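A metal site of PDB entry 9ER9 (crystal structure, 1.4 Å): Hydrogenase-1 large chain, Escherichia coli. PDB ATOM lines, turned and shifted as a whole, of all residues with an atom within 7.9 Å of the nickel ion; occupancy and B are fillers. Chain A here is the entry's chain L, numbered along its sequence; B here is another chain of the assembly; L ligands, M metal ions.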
ATOM      1  N   GLU A  28      20.604 -12.048  27.371  1.00  0.00           N
ATOM      2  CA  GLU A  28      21.700 -12.927  27.046  1.00  0.00           C
ATOM      3  C   GLU A  28      22.477 -13.278  28.319  1.00  0.00           C
ATOM      4  O   GLU A  28      22.858 -12.377  29.093  1.00  0.00           O
ATOM      5  CB  GLU A  28      22.649 -12.267  26.025  1.00  0.00           C
ATOM      6  CG  GLU A  28      23.633 -13.242  25.425  1.00  0.00           C
ATOM      7  CD  GLU A  28      24.718 -13.694  26.351  1.00  0.00           C
ATOM      8  OE1 GLU A  28      25.089 -12.848  27.185  1.00  0.00           O
ATOM      9  OE2 GLU A  28      25.096 -14.906  26.339  1.00  0.00           O
ATOM     10  N   GLU A  73      34.967 -12.567  18.860  1.00  0.00           N
ATOM     11  CA  GLU A  73      33.616 -12.584  18.310  1.00  0.00           C
ATOM     12  C   GLU A  73      32.735 -13.452  19.210  1.00  0.00           C
ATOM     13  O   GLU A  73      31.596 -13.112  19.416  1.00  0.00           O
ATOM     14  CB  GLU A  73      33.570 -13.043  16.858  1.00  0.00           C
ATOM     15  CG  GLU A  73      32.199 -12.841  16.217  1.00  0.00           C
ATOM     16  CD  GLU A  73      32.176 -12.980  14.703  1.00  0.00           C
ATOM     17  OE1 GLU A  73      32.663 -14.002  14.206  1.00  0.00           O
ATOM     18  OE2 GLU A  73      31.693 -12.078  14.035  1.00  0.00           O
ATOM     19  N   ILE A  75      32.720 -13.645  22.326  1.00  0.00           N
ATOM     20  CA  ILE A  75      32.258 -13.033  23.569  1.00  0.00           C
ATOM     21  C   ILE A  75      30.734 -13.058  23.572  1.00  0.00           C
ATOM     22  O   ILE A  75      30.109 -13.234  24.600  1.00  0.00           O
ATOM     23  CB  ILE A  75      32.822 -11.595  23.735  1.00  0.00           C
ATOM     24  CG1 ILE A  75      34.297 -11.662  24.094  1.00  0.00           C
ATOM     25  CG2 ILE A  75      31.999 -10.848  24.754  1.00  0.00           C
ATOM     26  CD1 ILE A  75      35.026 -10.344  23.991  1.00  0.00           C
ATOM     27  N   CYS A  76      30.125 -12.918  22.357  1.00  0.00           N
ATOM     28  CA  CYS A  76      28.679 -12.834  22.316  1.00  0.00           C
ATOM     29  C   CYS A  76      28.047 -13.201  20.968  1.00  0.00           C
ATOM     30  O   CYS A  76      28.486 -12.719  19.938  1.00  0.00           O
ATOM     31  CB  CYS A  76      28.217 -11.429  22.647  1.00  0.00           C
ATOM     32  SG  CYS A  76      26.429 -11.318  22.883  1.00  0.00           S
ATOM     33  N   GLY A  77      27.016 -14.061  21.033  1.00  0.00           N
ATOM     34  CA  GLY A  77      26.329 -14.576  19.861  1.00  0.00           C
ATOM     35  C   GLY A  77      25.090 -13.745  19.514  1.00  0.00           C
ATOM     36  O   GLY A  77      24.512 -13.904  18.445  1.00  0.00           O
ATOM     37  N   VAL A  78      24.687 -12.872  20.447  1.00  0.00           N
ATOM     38  CA  VAL A  78      23.567 -11.962  20.265  1.00  0.00           C
ATOM     39  C   VAL A  78      24.081 -10.715  19.560  1.00  0.00           C
ATOM     40  O   VAL A  78      23.657 -10.464  18.442  1.00  0.00           O
ATOM     41  CB  VAL A  78      22.868 -11.638  21.581  1.00  0.00           C
ATOM     42  CG1 VAL A  78      21.715 -10.687  21.361  1.00  0.00           C
ATOM     43  CG2 VAL A  78      22.387 -12.894  22.251  1.00  0.00           C
ATOM     44  N   CYS A  79      25.065 -10.022  20.136  1.00  0.00           N
ATOM     45  CA  CYS A  79      25.750  -8.926  19.431  1.00  0.00           C
ATOM     46  C   CYS A  79      26.866  -9.503  18.562  1.00  0.00           C
ATOM     47  O   CYS A  79      27.987  -9.006  18.529  1.00  0.00           O
ATOM     48  CB  CYS A  79      26.202  -7.797  20.363  1.00  0.00           C
ATOM     49  SG  CYS A  79      27.319  -8.312  21.686  1.00  0.00           S
ATOM     50  N   THR A  80      26.500 -10.507  17.745  1.00  0.00           N
ATOM     51  CA  THR A  80      27.486 -11.224  16.949  1.00  0.00           C
ATOM     52  C   THR A  80      28.076 -10.317  15.869  1.00  0.00           C
ATOM     53  O   THR A  80      27.365  -9.730  15.064  1.00  0.00           O
ATOM     54  CB  THR A  80      26.889 -12.494  16.342  1.00  0.00           C
ATOM     55  OG1 THR A  80      27.950 -13.189  15.664  1.00  0.00           O
ATOM     56  CG2 THR A  80      25.773 -12.237  15.357  1.00  0.00           C
ATOM     57  N   VAL A  82      30.128  -7.647  16.528  1.00  0.00           N
ATOM     58  CA  VAL A  82      30.566  -6.327  16.984  1.00  0.00           C
ATOM     59  C   VAL A  82      31.952  -6.417  17.618  1.00  0.00           C
ATOM     60  O   VAL A  82      32.781  -5.506  17.431  1.00  0.00           O
ATOM     61  CB  VAL A  82      29.556  -5.652  17.932  1.00  0.00           C
ATOM     62  CG1 VAL A  82      29.540  -6.246  19.344  1.00  0.00           C
ATOM     63  CG2 VAL A  82      29.852  -4.186  17.977  1.00  0.00           C
ATOM     64  N   HIS A  83      32.250  -7.537  18.277  1.00  0.00           N
ATOM     65  CA  HIS A  83      33.569  -7.741  18.874  1.00  0.00           C
ATOM     66  C   HIS A  83      34.617  -7.997  17.803  1.00  0.00           C
ATOM     67  O   HIS A  83      35.802  -7.690  17.980  1.00  0.00           O
ATOM     68  CB  HIS A  83      33.536  -8.833  19.937  1.00  0.00           C
ATOM     69  CG  HIS A  83      32.784  -8.416  21.146  1.00  0.00           C
ATOM     70  ND1 HIS A  83      33.351  -7.545  22.067  1.00  0.00           N
ATOM     71  CD2 HIS A  83      31.592  -8.791  21.629  1.00  0.00           C
ATOM     72  CE1 HIS A  83      32.490  -7.397  23.089  1.00  0.00           C
ATOM     73  NE2 HIS A  83      31.396  -8.121  22.822  1.00  0.00           N
ATOM     74  N   LEU A 114      23.547  -5.737  12.095  1.00  0.00           N
ATOM     75  CA  LEU A 114      23.476  -6.187  13.479  1.00  0.00           C
ATOM     76  C   LEU A 114      22.520  -5.309  14.286  1.00  0.00           C
ATOM     77  O   LEU A 114      21.660  -5.801  15.024  1.00  0.00           O
ATOM     78  CB  LEU A 114      24.879  -6.273  14.116  1.00  0.00           C
ATOM     79  CG  LEU A 114      24.846  -6.735  15.575  1.00  0.00           C
ATOM     80  CD1 LEU A 114      24.300  -8.192  15.693  1.00  0.00           C
ATOM     81  CD2 LEU A 114      26.223  -6.636  16.231  1.00  0.00           C
ATOM     82  N   ASP A 118      19.435  -7.177  16.001  1.00  0.00           N
ATOM     83  CA  ASP A 118      19.510  -7.231  17.431  1.00  0.00           C
ATOM     84  C   ASP A 118      18.386  -6.436  18.084  1.00  0.00           C
ATOM     85  O   ASP A 118      17.630  -6.948  18.969  1.00  0.00           O
ATOM     86  CB  ASP A 118      20.906  -6.757  17.838  1.00  0.00           C
ATOM     87  CG  ASP A 118      21.316  -7.166  19.249  1.00  0.00           C
ATOM     88  OD1 ASP A 118      20.418  -7.283  20.106  1.00  0.00           O
ATOM     89  OD2 ASP A 118      22.557  -7.359  19.467  1.00  0.00           O
ATOM     90  N   ALA A 507      28.157  -0.780  19.911  1.00  0.00           N
ATOM     91  CA  ALA A 507      27.386  -2.010  19.826  1.00  0.00           C
ATOM     92  C   ALA A 507      25.921  -1.699  20.069  1.00  0.00           C
ATOM     93  O   ALA A 507      25.535  -0.631  20.579  1.00  0.00           O
ATOM     94  CB  ALA A 507      27.941  -2.971  20.840  1.00  0.00           C
ATOM     95  N   PRO A 508      25.000  -2.637  19.748  1.00  0.00           N
ATOM     96  CA  PRO A 508      23.574  -2.403  20.011  1.00  0.00           C
ATOM     97  C   PRO A 508      23.306  -1.931  21.442  1.00  0.00           C
ATOM     98  O   PRO A 508      22.396  -1.146  21.638  1.00  0.00           O
ATOM     99  CB  PRO A 508      22.970  -3.793  19.764  1.00  0.00           C
ATOM    100  CG  PRO A 508      23.860  -4.316  18.638  1.00  0.00           C
ATOM    101  CD  PRO A 508      25.257  -3.864  18.971  1.00  0.00           C
ATOM    102  N   ARG A 509      24.125  -2.353  22.423  1.00  0.00           N
ATOM    103  CA  ARG A 509      23.881  -2.015  23.836  1.00  0.00           C
ATOM    104  C   ARG A 509      24.693  -0.829  24.344  1.00  0.00           C
ATOM    105  O   ARG A 509      24.464  -0.455  25.500  1.00  0.00           O
ATOM    106  CB  ARG A 509      24.087  -3.270  24.684  1.00  0.00           C
ATOM    107  CG  ARG A 509      23.029  -4.339  24.392  1.00  0.00           C
ATOM    108  CD  ARG A 509      23.437  -5.729  24.791  1.00  0.00           C
ATOM    109  NE  ARG A 509      22.382  -6.636  24.366  1.00  0.00           N
ATOM    110  CZ  ARG A 509      22.205  -7.061  23.120  1.00  0.00           C
ATOM    111  NH1 ARG A 509      23.111  -6.848  22.184  1.00  0.00           N
ATOM    112  NH2 ARG A 509      21.107  -7.737  22.846  1.00  0.00           N
ATOM    113  N   VAL A 530      32.969  -3.536  27.788  1.00  0.00           N
ATOM    114  CA  VAL A 530      31.831  -3.777  26.912  1.00  0.00           C
ATOM    115  C   VAL A 530      30.622  -3.020  27.454  1.00  0.00           C
ATOM    116  O   VAL A 530      30.568  -2.646  28.645  1.00  0.00           O
ATOM    117  CB  VAL A 530      31.642  -5.299  26.854  1.00  0.00           C
ATOM    118  CG1 VAL A 530      30.614  -5.754  25.840  1.00  0.00           C
ATOM    119  CG2 VAL A 530      32.990  -5.933  26.571  1.00  0.00           C
ATOM    120  N   PRO A 531      29.618  -2.671  26.625  1.00  0.00           N
ATOM    121  CA  PRO A 531      28.543  -1.830  27.114  1.00  0.00           C
ATOM    122  C   PRO A 531      27.854  -2.332  28.378  1.00  0.00           C
ATOM    123  O   PRO A 531      27.580  -1.555  29.296  1.00  0.00           O
ATOM    124  CB  PRO A 531      27.596  -1.590  25.926  1.00  0.00           C
ATOM    125  CG  PRO A 531      28.135  -2.479  24.804  1.00  0.00           C
ATOM    126  CD  PRO A 531      29.562  -2.848  25.176  1.00  0.00           C
ATOM    127  N   THR A 532      27.524  -3.618  28.467  1.00  0.00           N
ATOM    128  CA  THR A 532      26.838  -4.114  29.641  1.00  0.00           C
ATOM    129  C   THR A 532      27.799  -4.131  30.845  1.00  0.00           C
ATOM    130  O   THR A 532      27.353  -4.077  32.004  1.00  0.00           O
ATOM    131  CB  THR A 532      26.140  -5.448  29.367  1.00  0.00           C
ATOM    132  OG1 THR A 532      25.180  -5.234  28.324  1.00  0.00           O
ATOM    133  CG2 THR A 532      25.419  -5.978  30.585  1.00  0.00           C
ATOM    134  N   ASP A 574      18.539  -3.898  27.701  1.00  0.00           N
ATOM    135  CA  ASP A 574      18.966  -4.998  26.846  1.00  0.00           C
ATOM    136  C   ASP A 574      20.228  -5.680  27.386  1.00  0.00           C
ATOM    137  O   ASP A 574      21.298  -5.647  26.759  1.00  0.00           O
ATOM    138  CB  ASP A 574      19.089  -4.466  25.435  1.00  0.00           C
ATOM    139  CG  ASP A 574      19.437  -5.440  24.346  1.00  0.00           C
ATOM    140  OD1 ASP A 574      19.357  -6.668  24.581  1.00  0.00           O
ATOM    141  OD2 ASP A 574      19.831  -4.914  23.271  1.00  0.00           O
ATOM    142  N   PRO A 575      20.207  -6.258  28.608  1.00  0.00           N
ATOM    143  CA  PRO A 575      21.431  -6.805  29.204  1.00  0.00           C
ATOM    144  C   PRO A 575      22.057  -7.922  28.378  1.00  0.00           C
ATOM    145  O   PRO A 575      21.367  -8.873  27.970  1.00  0.00           O
ATOM    146  CB  PRO A 575      20.956  -7.381  30.557  1.00  0.00           C
ATOM    147  CG  PRO A 575      19.707  -6.593  30.844  1.00  0.00           C
ATOM    148  CD  PRO A 575      19.057  -6.418  29.484  1.00  0.00           C
ATOM    149  N   CYS A 576      23.375  -7.825  28.184  1.00  0.00           N
ATOM    150  CA  CYS A 576      24.133  -8.892  27.556  1.00  0.00           C
ATOM    151  C   CYS A 576      25.229  -9.320  28.550  1.00  0.00           C
ATOM    152  O   CYS A 576      26.273  -8.682  28.645  1.00  0.00           O
ATOM    153  CB  CYS A 576      24.714  -8.442  26.227  1.00  0.00           C
ATOM    154  SG  CYS A 576      25.322  -9.862  25.259  1.00  0.00           S
ATOM    155  N   LEU A 577      24.974 -10.409  29.277  1.00  0.00           N
ATOM    156  CA  LEU A 577      25.839 -10.739  30.408  1.00  0.00           C
ATOM    157  C   LEU A 577      27.141 -11.391  29.971  1.00  0.00           C
ATOM    158  O   LEU A 577      28.159 -11.229  30.626  1.00  0.00           O
ATOM    159  CB  LEU A 577      25.075 -11.567  31.437  1.00  0.00           C
ATOM    160  CG  LEU A 577      24.239 -10.732  32.411  1.00  0.00           C
ATOM    161  CD1 LEU A 577      25.144 -10.022  33.417  1.00  0.00           C
ATOM    162  CD2 LEU A 577      23.334  -9.720  31.717  1.00  0.00           C
ATOM    163  N   ALA A 578      27.116 -12.188  28.898  1.00  0.00           N
ATOM    164  CA  ALA A 578      28.334 -12.796  28.367  1.00  0.00           C
ATOM    165  C   ALA A 578      29.255 -11.683  27.867  1.00  0.00           C
ATOM    166  O   ALA A 578      30.461 -11.716  28.091  1.00  0.00           O
ATOM    167  CB  ALA A 578      28.018 -13.751  27.254  1.00  0.00           C
ATOM    168  N   CYS A 579      28.686 -10.646  27.221  1.00  0.00           N
ATOM    169  CA  CYS A 579      29.427  -9.443  26.880  1.00  0.00           C
ATOM    170  C   CYS A 579      30.045  -8.833  28.142  1.00  0.00           C
ATOM    171  O   CYS A 579      31.203  -8.449  28.127  1.00  0.00           O
ATOM    172  CB  CYS A 579      28.523  -8.405  26.214  1.00  0.00           C
ATOM    173  SG  CYS A 579      28.560  -8.516  24.401  1.00  0.00           S
ATOM    174  N   SER A 580      29.234  -8.657  29.181  1.00  0.00           N
ATOM    175  CA  SER A 580      29.624  -7.830  30.298  1.00  0.00           C
ATOM    176  C   SER A 580      30.856  -8.402  30.985  1.00  0.00           C
ATOM    177  O   SER A 580      31.646  -7.660  31.557  1.00  0.00           O
ATOM    178  CB  SER A 580      28.454  -7.679  31.255  1.00  0.00           C
ATOM    179  OG  SER A 580      28.266  -8.842  32.045  1.00  0.00           O
ATOM    180  N   CYS B  17      27.939 -18.042  24.727  1.00  0.00           N
ATOM    181  CA  CYS B  17      27.741 -16.739  24.133  1.00  0.00           C
ATOM    182  C   CYS B  17      26.312 -16.570  23.591  1.00  0.00           C
ATOM    183  O   CYS B  17      25.996 -15.497  23.160  1.00  0.00           O
ATOM    184  CB  CYS B  17      28.759 -16.464  23.037  1.00  0.00           C
ATOM    185  SG  CYS B  17      28.336 -17.161  21.397  1.00  0.00           S
HETATM  186 FE1  LIG L   1      27.347  -6.863  23.458  1.00  0.00          FE
HETATM  187  C1  LIG L   1      27.038  -6.029  25.112  1.00  0.00           C
HETATM  188  N1  LIG L   1      26.857  -5.437  26.071  1.00  0.00           N
HETATM  189  C2  LIG L   1      26.278  -5.632  22.703  1.00  0.00           C
HETATM  190  N2  LIG L   1      25.542  -4.868  22.118  1.00  0.00           N
HETATM  191  C3  LIG L   1      28.729  -5.820  23.015  1.00  0.00           C
HETATM  192  O1  LIG L   1      29.654  -5.183  22.707  1.00  0.00           O
HETATM  193 NI    NI M   1      26.314  -9.198  23.508  1.00  0.00          NI
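The side-chain sulfur (SG) of Cys 579 is bound to an iron atom (FE1) of the ligand, at 2.3 Å.
The backbone NH (N) of Arg 509 lies within hydrogen-bond range of a nitrogen (N2) of the ligand (2.9 Å).
The backbone NH of Thr 532 sits at hydrogen-bond distance from a nitrogen (N1) of the ligand.
The side-chain sulfur (SG) of Cys 79 is bound to an iron atom (FE1) of the ligand (2.3 Å).
A nitrogen (N1) of the ligand sits at hydrogen-bond distance from the side-chain hydroxyl (OG1) of Thr 532 (2.8 Å).
A ring nitrogen (NE2) of His 83 sits at hydrogen-bond distance from an oxygen (O1) of the ligand (3.4 Å).
The guanidinium group (NH1) of Arg 509 lies within hydrogen-bond range of a nitrogen (N2) of the ligand (3.1 Å).
SG of Cys 576 lies close to OE1 of Glu 28, at 3.6 Å.
A ring nitrogen (NE2) of His 83 lies close to the side-chain sulfur of Cys 579.
SG of Cys 76 sits close to N of Val 78, at 3.4 Å.
N of Cys 576 is in hydrogen-bond range of OG1 of Thr 532, at 3.2 Å.
SG of Cys 576 is bound to the nickel ion (2.1 Å).
The nickel ion is bound by the side-chain sulfur (SG) of Cys 76 (2.2 Å).
The nickel ion is bound by the side-chain sulfur (SG) of Cys 79, 2.3 Å away.
The nickel ion is bound by the side-chain sulfur (SG) of Cys 579 (2.5 Å).
The nickel ion has four donor atoms within binding distance.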
